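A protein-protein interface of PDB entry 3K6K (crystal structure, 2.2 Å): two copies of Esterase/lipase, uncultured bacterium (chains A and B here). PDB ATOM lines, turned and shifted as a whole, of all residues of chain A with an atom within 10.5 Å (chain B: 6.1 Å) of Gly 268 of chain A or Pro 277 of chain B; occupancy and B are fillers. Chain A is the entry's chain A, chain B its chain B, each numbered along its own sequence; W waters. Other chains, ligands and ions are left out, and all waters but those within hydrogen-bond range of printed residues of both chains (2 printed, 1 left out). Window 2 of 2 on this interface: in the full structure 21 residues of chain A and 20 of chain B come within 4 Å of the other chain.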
ATOM      1  N   LYS A 171      -9.987 -20.228  -9.185  1.00  0.00           N
ATOM      2  CA  LYS A 171     -11.158 -21.119  -9.259  1.00  0.00           C
ATOM      3  C   LYS A 171     -10.901 -22.269 -10.240  1.00  0.00           C
ATOM      4  O   LYS A 171     -11.105 -23.419  -9.840  1.00  0.00           O
ATOM      5  CB  LYS A 171     -12.434 -20.361  -9.652  1.00  0.00           C
ATOM      6  CG  LYS A 171     -13.806 -21.044  -9.278  1.00  0.00           C
ATOM      7  CD  LYS A 171     -15.047 -20.181  -9.703  1.00  0.00           C
ATOM      8  CE  LYS A 171     -15.256 -20.256 -11.226  1.00  0.00           C
ATOM      9  NZ  LYS A 171     -15.842 -19.017 -11.934  1.00  0.00           N
ATOM     10  N   ALA A 235     -15.884 -12.505 -18.825  1.00  0.00           N
ATOM     11  CA  ALA A 235     -15.739 -13.870 -18.236  1.00  0.00           C
ATOM     12  C   ALA A 235     -17.058 -14.640 -17.971  1.00  0.00           C
ATOM     13  O   ALA A 235     -18.154 -14.097 -18.094  1.00  0.00           O
ATOM     14  CB  ALA A 235     -14.901 -13.829 -16.956  1.00  0.00           C
ATOM     15  N   ASP A 236     -16.922 -15.912 -17.618  1.00  0.00           N
ATOM     16  CA  ASP A 236     -17.961 -16.641 -16.928  1.00  0.00           C
ATOM     17  C   ASP A 236     -17.642 -16.387 -15.475  1.00  0.00           C
ATOM     18  O   ASP A 236     -16.688 -16.916 -14.908  1.00  0.00           O
ATOM     19  CB  ASP A 236     -17.919 -18.135 -17.239  1.00  0.00           C
ATOM     20  CG  ASP A 236     -18.761 -18.955 -16.278  1.00  0.00           C
ATOM     21  OD1 ASP A 236     -19.552 -18.351 -15.515  1.00  0.00           O
ATOM     22  OD2 ASP A 236     -18.611 -20.204 -16.276  1.00  0.00           O
ATOM     23  N   LEU A 237     -18.439 -15.537 -14.860  1.00  0.00           N
ATOM     24  CA  LEU A 237     -18.067 -15.038 -13.546  1.00  0.00           C
ATOM     25  C   LEU A 237     -18.703 -15.846 -12.454  1.00  0.00           C
ATOM     26  O   LEU A 237     -18.661 -15.428 -11.294  1.00  0.00           O
ATOM     27  CB  LEU A 237     -18.511 -13.580 -13.466  1.00  0.00           C
ATOM     28  CG  LEU A 237     -17.640 -12.645 -14.319  1.00  0.00           C
ATOM     29  CD1 LEU A 237     -18.399 -11.523 -14.978  1.00  0.00           C
ATOM     30  CD2 LEU A 237     -16.540 -12.090 -13.396  1.00  0.00           C
ATOM     31  N   SER A 238     -19.379 -16.935 -12.829  1.00  0.00           N
ATOM     32  CA  SER A 238     -20.032 -17.866 -11.878  1.00  0.00           C
ATOM     33  C   SER A 238     -19.155 -18.283 -10.682  1.00  0.00           C
ATOM     34  O   SER A 238     -18.001 -18.706 -10.842  1.00  0.00           O
ATOM     35  CB  SER A 238     -20.428 -19.174 -12.613  1.00  0.00           C
ATOM     36  OG  SER A 238     -21.228 -18.916 -13.753  1.00  0.00           O
ATOM     37  N   GLY A 239     -19.689 -18.174  -9.489  1.00  0.00           N
ATOM     38  CA  GLY A 239     -19.072 -18.847  -8.335  1.00  0.00           C
ATOM     39  C   GLY A 239     -18.021 -18.015  -7.650  1.00  0.00           C
ATOM     40  O   GLY A 239     -17.441 -18.416  -6.601  1.00  0.00           O
ATOM     41  N   LEU A 240     -17.763 -16.841  -8.225  1.00  0.00           N
ATOM     42  CA  LEU A 240     -17.005 -15.809  -7.503  1.00  0.00           C
ATOM     43  C   LEU A 240     -17.728 -15.378  -6.232  1.00  0.00           C
ATOM     44  O   LEU A 240     -18.969 -15.419  -6.194  1.00  0.00           O
ATOM     45  CB  LEU A 240     -16.743 -14.635  -8.420  1.00  0.00           C
ATOM     46  CG  LEU A 240     -15.725 -14.949  -9.535  1.00  0.00           C
ATOM     47  CD1 LEU A 240     -15.432 -13.678 -10.246  1.00  0.00           C
ATOM     48  CD2 LEU A 240     -14.410 -15.565  -9.041  1.00  0.00           C
ATOM     49  N   PRO A 241     -16.967 -15.004  -5.195  1.00  0.00           N
ATOM     50  CA  PRO A 241     -17.399 -14.552  -3.872  1.00  0.00           C
ATOM     51  C   PRO A 241     -17.926 -13.106  -3.840  1.00  0.00           C
ATOM     52  O   PRO A 241     -17.778 -12.347  -4.826  1.00  0.00           O
ATOM     53  CB  PRO A 241     -16.122 -14.641  -3.029  1.00  0.00           C
ATOM     54  CG  PRO A 241     -15.001 -14.788  -3.951  1.00  0.00           C
ATOM     55  CD  PRO A 241     -15.496 -15.035  -5.330  1.00  0.00           C
ATOM     56  N   GLU A 242     -18.556 -12.701  -2.751  1.00  0.00           N
ATOM     57  CA  GLU A 242     -19.208 -11.381  -2.768  1.00  0.00           C
ATOM     58  C   GLU A 242     -18.306 -10.191  -3.090  1.00  0.00           C
ATOM     59  O   GLU A 242     -17.176 -10.105  -2.626  1.00  0.00           O
ATOM     60  CB  GLU A 242     -20.060 -11.131  -1.565  1.00  0.00           C
ATOM     61  CG  GLU A 242     -19.471 -11.557  -0.281  1.00  0.00           C
ATOM     62  CD  GLU A 242     -20.547 -11.728   0.812  1.00  0.00           C
ATOM     63  OE1 GLU A 242     -21.504 -10.927   0.860  1.00  0.00           O
ATOM     64  OE2 GLU A 242     -20.404 -12.634   1.648  1.00  0.00           O
ATOM     65  N   MET A 243     -18.845  -9.267  -3.879  1.00  0.00           N
ATOM     66  CA  MET A 243     -18.091  -8.160  -4.397  1.00  0.00           C
ATOM     67  C   MET A 243     -18.614  -6.843  -3.819  1.00  0.00           C
ATOM     68  O   MET A 243     -19.836  -6.641  -3.724  1.00  0.00           O
ATOM     69  CB  MET A 243     -18.240  -8.143  -5.902  1.00  0.00           C
ATOM     70  CG  MET A 243     -17.511  -9.253  -6.656  1.00  0.00           C
ATOM     71  SD  MET A 243     -17.846  -8.971  -8.417  1.00  0.00           S
ATOM     72  CE  MET A 243     -16.871 -10.193  -9.310  1.00  0.00           C
ATOM     73  N   LEU A 260     -19.252  -4.640 -14.903  1.00  0.00           N
ATOM     74  CA  LEU A 260     -18.949  -5.762 -14.044  1.00  0.00           C
ATOM     75  C   LEU A 260     -20.080  -6.090 -13.062  1.00  0.00           C
ATOM     76  O   LEU A 260     -20.287  -7.265 -12.680  1.00  0.00           O
ATOM     77  CB  LEU A 260     -17.711  -5.461 -13.232  1.00  0.00           C
ATOM     78  CG  LEU A 260     -16.691  -6.505 -12.716  1.00  0.00           C
ATOM     79  CD1 LEU A 260     -16.383  -6.277 -11.212  1.00  0.00           C
ATOM     80  CD2 LEU A 260     -16.855  -7.991 -13.123  1.00  0.00           C
ATOM     81  N   ALA A 261     -20.761  -5.070 -12.574  1.00  0.00           N
ATOM     82  CA  ALA A 261     -21.885  -5.323 -11.660  1.00  0.00           C
ATOM     83  C   ALA A 261     -22.996  -6.028 -12.477  1.00  0.00           C
ATOM     84  O   ALA A 261     -23.539  -7.033 -12.043  1.00  0.00           O
ATOM     85  CB  ALA A 261     -22.382  -4.004 -11.005  1.00  0.00           C
ATOM     86  N   GLU A 262     -23.316  -5.504 -13.665  1.00  0.00           N
ATOM     87  CA  GLU A 262     -24.307  -6.150 -14.495  1.00  0.00           C
ATOM     88  C   GLU A 262     -24.034  -7.667 -14.594  1.00  0.00           C
ATOM     89  O   GLU A 262     -24.891  -8.522 -14.195  1.00  0.00           O
ATOM     90  CB  GLU A 262     -24.327  -5.529 -15.897  1.00  0.00           C
ATOM     91  CG  GLU A 262     -25.484  -5.979 -16.755  1.00  0.00           C
ATOM     92  CD  GLU A 262     -25.547  -5.182 -17.986  1.00  0.00           C
ATOM     93  OE1 GLU A 262     -26.310  -4.228 -18.053  1.00  0.00           O
ATOM     94  OE2 GLU A 262     -24.749  -5.441 -18.887  1.00  0.00           O
ATOM     95  N   ARG A 263     -22.822  -7.994 -15.033  1.00  0.00           N
ATOM     96  CA  ARG A 263     -22.487  -9.317 -15.445  1.00  0.00           C
ATOM     97  C   ARG A 263     -22.175 -10.183 -14.237  1.00  0.00           C
ATOM     98  O   ARG A 263     -22.522 -11.392 -14.161  1.00  0.00           O
ATOM     99  CB  ARG A 263     -21.319  -9.314 -16.455  1.00  0.00           C
ATOM    100  CG  ARG A 263     -21.543  -8.359 -17.694  1.00  0.00           C
ATOM    101  CD  ARG A 263     -22.903  -8.635 -18.431  1.00  0.00           C
ATOM    102  NE  ARG A 263     -23.082  -7.724 -19.578  1.00  0.00           N
ATOM    103  CZ  ARG A 263     -22.491  -7.873 -20.770  1.00  0.00           C
ATOM    104  NH1 ARG A 263     -21.702  -8.923 -20.989  1.00  0.00           N
ATOM    105  NH2 ARG A 263     -22.680  -6.974 -21.744  1.00  0.00           N
ATOM    106  N   ALA A 264     -21.531  -9.606 -13.259  1.00  0.00           N
ATOM    107  CA  ALA A 264     -21.292 -10.445 -12.092  1.00  0.00           C
ATOM    108  C   ALA A 264     -22.683 -10.802 -11.434  1.00  0.00           C
ATOM    109  O   ALA A 264     -22.930 -11.960 -11.053  1.00  0.00           O
ATOM    110  CB  ALA A 264     -20.344  -9.820 -11.183  1.00  0.00           C
ATOM    111  N   GLY A 265     -23.607  -9.849 -11.384  1.00  0.00           N
ATOM    112  CA  GLY A 265     -24.883 -10.081 -10.700  1.00  0.00           C
ATOM    113  C   GLY A 265     -25.657 -11.142 -11.448  1.00  0.00           C
ATOM    114  O   GLY A 265     -26.225 -12.015 -10.827  1.00  0.00           O
ATOM    115  N   ALA A 266     -25.596 -11.102 -12.781  1.00  0.00           N
ATOM    116  CA  ALA A 266     -26.360 -12.020 -13.641  1.00  0.00           C
ATOM    117  C   ALA A 266     -25.767 -13.414 -13.607  1.00  0.00           C
ATOM    118  O   ALA A 266     -26.464 -14.389 -13.932  1.00  0.00           O
ATOM    119  CB  ALA A 266     -26.397 -11.505 -15.117  1.00  0.00           C
ATOM    120  N   ALA A 267     -24.483 -13.494 -13.263  1.00  0.00           N
ATOM    121  CA  ALA A 267     -23.793 -14.763 -13.038  1.00  0.00           C
ATOM    122  C   ALA A 267     -24.066 -15.283 -11.633  1.00  0.00           C
ATOM    123  O   ALA A 267     -23.551 -16.323 -11.229  1.00  0.00           O
ATOM    124  CB  ALA A 267     -22.305 -14.607 -13.262  1.00  0.00           C
ATOM    125  N   GLY A 268     -24.868 -14.548 -10.870  1.00  0.00           N
ATOM    126  CA  GLY A 268     -25.241 -15.002  -9.513  1.00  0.00           C
ATOM    127  C   GLY A 268     -24.224 -14.672  -8.443  1.00  0.00           C
ATOM    128  O   GLY A 268     -24.177 -15.334  -7.466  1.00  0.00           O
ATOM    129  N   VAL A 269     -23.416 -13.634  -8.650  1.00  0.00           N
ATOM    130  CA  VAL A 269     -22.453 -13.153  -7.645  1.00  0.00           C
ATOM    131  C   VAL A 269     -23.154 -12.054  -6.841  1.00  0.00           C
ATOM    132  O   VAL A 269     -23.893 -11.285  -7.422  1.00  0.00           O
ATOM    133  CB  VAL A 269     -21.162 -12.582  -8.369  1.00  0.00           C
ATOM    134  CG1 VAL A 269     -20.200 -11.980  -7.404  1.00  0.00           C
ATOM    135  CG2 VAL A 269     -20.443 -13.643  -9.096  1.00  0.00           C
ATOM    136  N   SER A 270     -22.957 -11.992  -5.524  1.00  0.00           N
ATOM    137  CA  SER A 270     -23.457 -10.830  -4.722  1.00  0.00           C
ATOM    138  C   SER A 270     -22.656  -9.605  -5.137  1.00  0.00           C
ATOM    139  O   SER A 270     -21.437  -9.699  -5.250  1.00  0.00           O
ATOM    140  CB  SER A 270     -23.258 -11.053  -3.247  1.00  0.00           C
ATOM    141  OG  SER A 270     -23.705  -9.937  -2.516  1.00  0.00           O
ATOM    142  N   VAL A 271     -23.319  -8.477  -5.406  1.00  0.00           N
ATOM    143  CA  VAL A 271     -22.573  -7.316  -5.804  1.00  0.00           C
ATOM    144  C   VAL A 271     -23.185  -6.091  -5.189  1.00  0.00           C
ATOM    145  O   VAL A 271     -24.401  -5.859  -5.266  1.00  0.00           O
ATOM    146  CB  VAL A 271     -22.506  -7.091  -7.352  1.00  0.00           C
ATOM    147  CG1 VAL A 271     -21.647  -5.864  -7.649  1.00  0.00           C
ATOM    148  CG2 VAL A 271     -21.877  -8.271  -8.077  1.00  0.00           C
ATOM    149  N   GLU A 272     -22.327  -5.297  -4.574  1.00  0.00           N
ATOM    150  CA  GLU A 272     -22.749  -4.008  -4.063  1.00  0.00           C
ATOM    151  C   GLU A 272     -21.827  -2.957  -4.608  1.00  0.00           C
ATOM    152  O   GLU A 272     -20.604  -3.055  -4.491  1.00  0.00           O
ATOM    153  CB  GLU A 272     -22.685  -4.011  -2.542  1.00  0.00           C
ATOM    154  CG  GLU A 272     -23.205  -5.282  -1.930  1.00  0.00           C
ATOM    155  CD  GLU A 272     -23.056  -5.305  -0.387  1.00  0.00           C
ATOM    156  OE1 GLU A 272     -22.566  -6.350   0.131  1.00  0.00           O
ATOM    157  OE2 GLU A 272     -23.413  -4.268   0.272  1.00  0.00           O
ATOM    158  N   ARG A 307     -17.373  -9.610   7.110  1.00  0.00           N
ATOM    159  CA  ARG A 307     -17.451 -10.890   6.360  1.00  0.00           C
ATOM    160  C   ARG A 307     -16.543 -11.854   7.066  1.00  0.00           C
ATOM    161  O   ARG A 307     -16.812 -13.041   7.119  1.00  0.00           O
ATOM    162  CB  ARG A 307     -17.085 -10.744   4.902  1.00  0.00           C
ATOM    163  CG  ARG A 307     -17.873  -9.663   4.263  1.00  0.00           C
ATOM    164  CD  ARG A 307     -18.468 -10.087   2.970  1.00  0.00           C
ATOM    165  NE  ARG A 307     -19.801  -9.522   2.616  1.00  0.00           N
ATOM    166  CZ  ARG A 307     -20.466  -8.474   3.155  1.00  0.00           C
ATOM    167  NH1 ARG A 307     -19.994  -7.740   4.175  1.00  0.00           N
ATOM    168  NH2 ARG A 307     -21.658  -8.157   2.627  1.00  0.00           N
ATOM    169  N   PRO B  18     -33.735 -20.491  -2.499  1.00  0.00           N
ATOM    170  CA  PRO B  18     -33.951 -19.594  -3.623  1.00  0.00           C
ATOM    171  C   PRO B  18     -34.218 -20.319  -4.949  1.00  0.00           C
ATOM    172  O   PRO B  18     -35.171 -19.952  -5.641  1.00  0.00           O
ATOM    173  CB  PRO B  18     -32.643 -18.821  -3.711  1.00  0.00           C
ATOM    174  CG  PRO B  18     -31.851 -19.188  -2.432  1.00  0.00           C
ATOM    175  CD  PRO B  18     -32.746 -19.941  -1.552  1.00  0.00           C
ATOM    176  N   ARG B 203     -35.155 -16.139 -17.698  1.00  0.00           N
ATOM    177  CA  ARG B 203     -34.905 -16.349 -16.331  1.00  0.00           C
ATOM    178  C   ARG B 203     -35.909 -15.588 -15.490  1.00  0.00           C
ATOM    179  O   ARG B 203     -36.017 -15.826 -14.297  1.00  0.00           O
ATOM    180  CB  ARG B 203     -33.510 -15.865 -16.029  1.00  0.00           C
ATOM    181  CG  ARG B 203     -32.409 -16.852 -16.318  1.00  0.00           C
ATOM    182  CD  ARG B 203     -31.378 -16.553 -15.278  1.00  0.00           C
ATOM    183  NE  ARG B 203     -30.100 -16.338 -15.873  1.00  0.00           N
ATOM    184  CZ  ARG B 203     -29.014 -15.900 -15.242  1.00  0.00           C
ATOM    185  NH1 ARG B 203     -29.005 -15.571 -13.952  1.00  0.00           N
ATOM    186  NH2 ARG B 203     -27.924 -15.769 -15.972  1.00  0.00           N
ATOM    187  N   GLY B 248     -32.837  -8.054  -8.172  1.00  0.00           N
ATOM    188  CA  GLY B 248     -32.451  -9.460  -8.055  1.00  0.00           C
ATOM    189  C   GLY B 248     -31.605  -9.786  -9.275  1.00  0.00           C
ATOM    190  O   GLY B 248     -31.642  -9.012 -10.259  1.00  0.00           O
ATOM    191  N   SER B 249     -30.873 -10.907  -9.235  1.00  0.00           N
ATOM    192  CA  SER B 249     -30.177 -11.431 -10.439  1.00  0.00           C
ATOM    193  C   SER B 249     -31.120 -11.877 -11.562  1.00  0.00           C
ATOM    194  O   SER B 249     -30.712 -11.869 -12.702  1.00  0.00           O
ATOM    195  CB  SER B 249     -29.242 -12.644 -10.106  1.00  0.00           C
ATOM    196  OG  SER B 249     -30.000 -13.712  -9.550  1.00  0.00           O
ATOM    197  N   GLU B 250     -32.350 -12.301 -11.253  1.00  0.00           N
ATOM    198  CA  GLU B 250     -33.126 -13.107 -12.171  1.00  0.00           C
ATOM    199  C   GLU B 250     -34.116 -12.234 -12.895  1.00  0.00           C
ATOM    200  O   GLU B 250     -35.343 -12.488 -12.921  1.00  0.00           O
ATOM    201  CB  GLU B 250     -33.841 -14.237 -11.391  1.00  0.00           C
ATOM    202  CG  GLU B 250     -32.848 -15.191 -10.739  1.00  0.00           C
ATOM    203  CD  GLU B 250     -31.773 -15.723 -11.726  1.00  0.00           C
ATOM    204  OE1 GLU B 250     -32.153 -16.528 -12.621  1.00  0.00           O
ATOM    205  OE2 GLU B 250     -30.565 -15.381 -11.571  1.00  0.00           O
ATOM    206  N   ILE B 275     -27.138  -6.026  -6.055  1.00  0.00           N
ATOM    207  CA  ILE B 275     -27.675  -7.140  -6.804  1.00  0.00           C
ATOM    208  C   ILE B 275     -27.665  -8.472  -6.006  1.00  0.00           C
ATOM    209  O   ILE B 275     -26.615  -8.945  -5.582  1.00  0.00           O
ATOM    210  CB  ILE B 275     -26.853  -7.310  -8.036  1.00  0.00           C
ATOM    211  CG1 ILE B 275     -26.619  -5.916  -8.659  1.00  0.00           C
ATOM    212  CG2 ILE B 275     -27.491  -8.368  -8.990  1.00  0.00           C
ATOM    213  CD1 ILE B 275     -25.762  -6.020  -9.948  1.00  0.00           C
ATOM    214  N   TRP B 276     -28.859  -9.072  -5.830  1.00  0.00           N
ATOM    215  CA  TRP B 276     -29.038 -10.260  -4.971  1.00  0.00           C
ATOM    216  C   TRP B 276     -29.094 -11.609  -5.688  1.00  0.00           C
ATOM    217  O   TRP B 276     -30.003 -11.832  -6.494  1.00  0.00           O
ATOM    218  CB  TRP B 276     -30.312 -10.071  -4.205  1.00  0.00           C
ATOM    219  CG  TRP B 276     -30.284  -8.840  -3.335  1.00  0.00           C
ATOM    220  CD1 TRP B 276     -30.394  -7.513  -3.745  1.00  0.00           C
ATOM    221  CD2 TRP B 276     -30.137  -8.817  -1.917  1.00  0.00           C
ATOM    222  NE1 TRP B 276     -30.354  -6.691  -2.639  1.00  0.00           N
ATOM    223  CE2 TRP B 276     -30.184  -7.461  -1.511  1.00  0.00           C
ATOM    224  CE3 TRP B 276     -29.991  -9.821  -0.937  1.00  0.00           C
ATOM    225  CZ2 TRP B 276     -30.071  -7.082  -0.168  1.00  0.00           C
ATOM    226  CZ3 TRP B 276     -29.879  -9.451   0.382  1.00  0.00           C
ATOM    227  CH2 TRP B 276     -29.919  -8.092   0.764  1.00  0.00           C
ATOM    228  N   PRO B 277     -28.140 -12.524  -5.404  1.00  0.00           N
ATOM    229  CA  PRO B 277     -28.150 -13.800  -6.136  1.00  0.00           C
ATOM    230  C   PRO B 277     -29.459 -14.567  -6.050  1.00  0.00           C
ATOM    231  O   PRO B 277     -30.078 -14.668  -4.980  1.00  0.00           O
ATOM    232  CB  PRO B 277     -27.012 -14.592  -5.496  1.00  0.00           C
ATOM    233  CG  PRO B 277     -26.026 -13.549  -5.216  1.00  0.00           C
ATOM    234  CD  PRO B 277     -26.830 -12.327  -4.758  1.00  0.00           C
ATOM    235  N   ASP B 278     -29.867 -15.065  -7.210  1.00  0.00           N
ATOM    236  CA  ASP B 278     -31.017 -16.001  -7.367  1.00  0.00           C
ATOM    237  C   ASP B 278     -32.354 -15.363  -7.026  1.00  0.00           C
ATOM    238  O   ASP B 278     -33.360 -16.082  -6.834  1.00  0.00           O
ATOM    239  CB  ASP B 278     -30.795 -17.323  -6.577  1.00  0.00           C
ATOM    240  CG  ASP B 278     -29.536 -18.107  -7.054  1.00  0.00           C
ATOM    241  OD1 ASP B 278     -29.219 -18.150  -8.247  1.00  0.00           O
ATOM    242  OD2 ASP B 278     -28.866 -18.738  -6.228  1.00  0.00           O
ATOM    243  N   MET B 279     -32.403 -14.028  -6.957  1.00  0.00           N
ATOM    244  CA  MET B 279     -33.678 -13.389  -6.579  1.00  0.00           C
ATOM    245  C   MET B 279     -34.384 -12.939  -7.842  1.00  0.00           C
ATOM    246  O   MET B 279     -33.753 -12.446  -8.734  1.00  0.00           O
ATOM    247  CB  MET B 279     -33.483 -12.219  -5.594  1.00  0.00           C
ATOM    248  CG  MET B 279     -33.035 -12.643  -4.148  1.00  0.00           C
ATOM    249  SD  MET B 279     -34.395 -13.491  -3.366  1.00  0.00           S
ATOM    250  CE  MET B 279     -33.585 -15.056  -2.917  1.00  0.00           C
ATOM    251  N   ALA B 292     -33.640 -13.884   1.630  1.00  0.00           N
ATOM    252  CA  ALA B 292     -32.948 -12.720   1.131  1.00  0.00           C
ATOM    253  C   ALA B 292     -33.894 -11.522   1.228  1.00  0.00           C
ATOM    254  O   ALA B 292     -33.489 -10.422   1.579  1.00  0.00           O
ATOM    255  CB  ALA B 292     -32.424 -12.931  -0.318  1.00  0.00           C
HETATM  256  O   HOH W   1     -26.062  -9.217  -2.740  1.00  0.00           O
HETATM  257  O   HOH W   2     -25.154 -14.580 -17.072  1.00  0.00           O
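NH1 of Arg 203 of chain B is in hydrogen-bond range of O of Ala 266 of chain A. The backbone NH (N) of Ile 275 of chain B sits at hydrogen-bond distance from the backbone carbonyl oxygen (O) of Val 271 of chain A (2.9 Å).
Glu 242 of chain A touches none of the printed residues of chain B. Of the printed residues of chain B, Gly 265 of chain A touches Ser 249 (3.2 Å) and Ile 275 (3.6 Å). Printed residues of chain B within 4 Å of Ala 266 of chain A: Arg 203 (2.8 Å). Of the printed residues of chain B, Gly 268 of chain A touches Pro 277 (3.4 Å). Of the printed residues of chain B, Val 269 of chain A touches Pro 277 (3.6 Å). Printed residues of chain B within 4 Å of Ser 270 of chain A: Ile 275 and Pro 277. Glu 272 of chain A touches none of the printed residues of chain B. Of the printed residues of chain A, Arg 203 of chain B touches Ala 266. Pro 277 of chain B touches just these residues of chain A: Gly 268 (3.4 Å), Val 269 (3.6 Å) and Ser 270 (3.5 Å). No residue of chain A comes within 4 Å of Met 279 of chain B. The nearest residue of chain B that does not touch Gly 268 of chain A is Ser 249 of chain B (4.7 Å). The nearest residue of chain A that does not touch Pro 277 of chain B is Val 271 of chain A (5.3 Å). The nearest printed residue of chain B that does not touch Ala 266 of chain A is Ser 249 of chain B (4.5 Å).
Among the printed residues, pairs that only touch across the chains: Gly 265 of chain A with Ser 249 of chain B (3.2 Å), Ala 261 of chain A with Ile 275 of chain B (3.2 Å), Gly 268 of chain A with Pro 277 of chain B (3.4 Å), Ser 270 of chain A with Pro 277 of chain B (3.5 Å), Gly 265 of chain A with Ile 275 of chain B (3.6 Å), Val 269 of chain A with Pro 277 of chain B (3.6 Å) and Ser 270 of chain A with Ile 275 of chain B (3.8 Å).
Hydrophobic or aromatic side chains of chain B that line the printed part of chain A: Ile 275 and Pro 277. Among the printed residues, 9 pairs touch across the chains.
The backbone carbonyl oxygen (O) of Ser 270 of chain A sits at hydrogen-bond distance from the backbone NH (N) of Met 243 of chain A (3.0 Å). O of Ala 264 of chain A sits at hydrogen-bond distance from N of Val 269 of chain A, at 3.0 Å. The side-chain hydroxyl of Ser 249 of chain B sits at hydrogen-bond distance from the side-chain carboxylate of Glu 250 of chain B (2.7 Å). The backbone carbonyl oxygen of Trp 276 of chain B is in hydrogen-bond range of the backbone NH of Ser 249 of chain B (3.0 Å). OG of Ser 249 of chain B is in hydrogen-bond range of N of Asp 278 of chain B. The backbone NH (N) of Ser 249 of chain B is in hydrogen-bond range of the backbone carbonyl oxygen (O) of Met 279 of chain B, at 3.3 Å.
No position is printed for both chains.
Water W1 bridges OG of Ser 270 of chain A (2.5 Å) and O of Ile 275 of chain B (2.9 Å). Water W2 bridges the guanidinium group (NH2) of Arg 203 of chain B and the backbone carbonyl oxygen (O) of Ala 266 of chain A.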
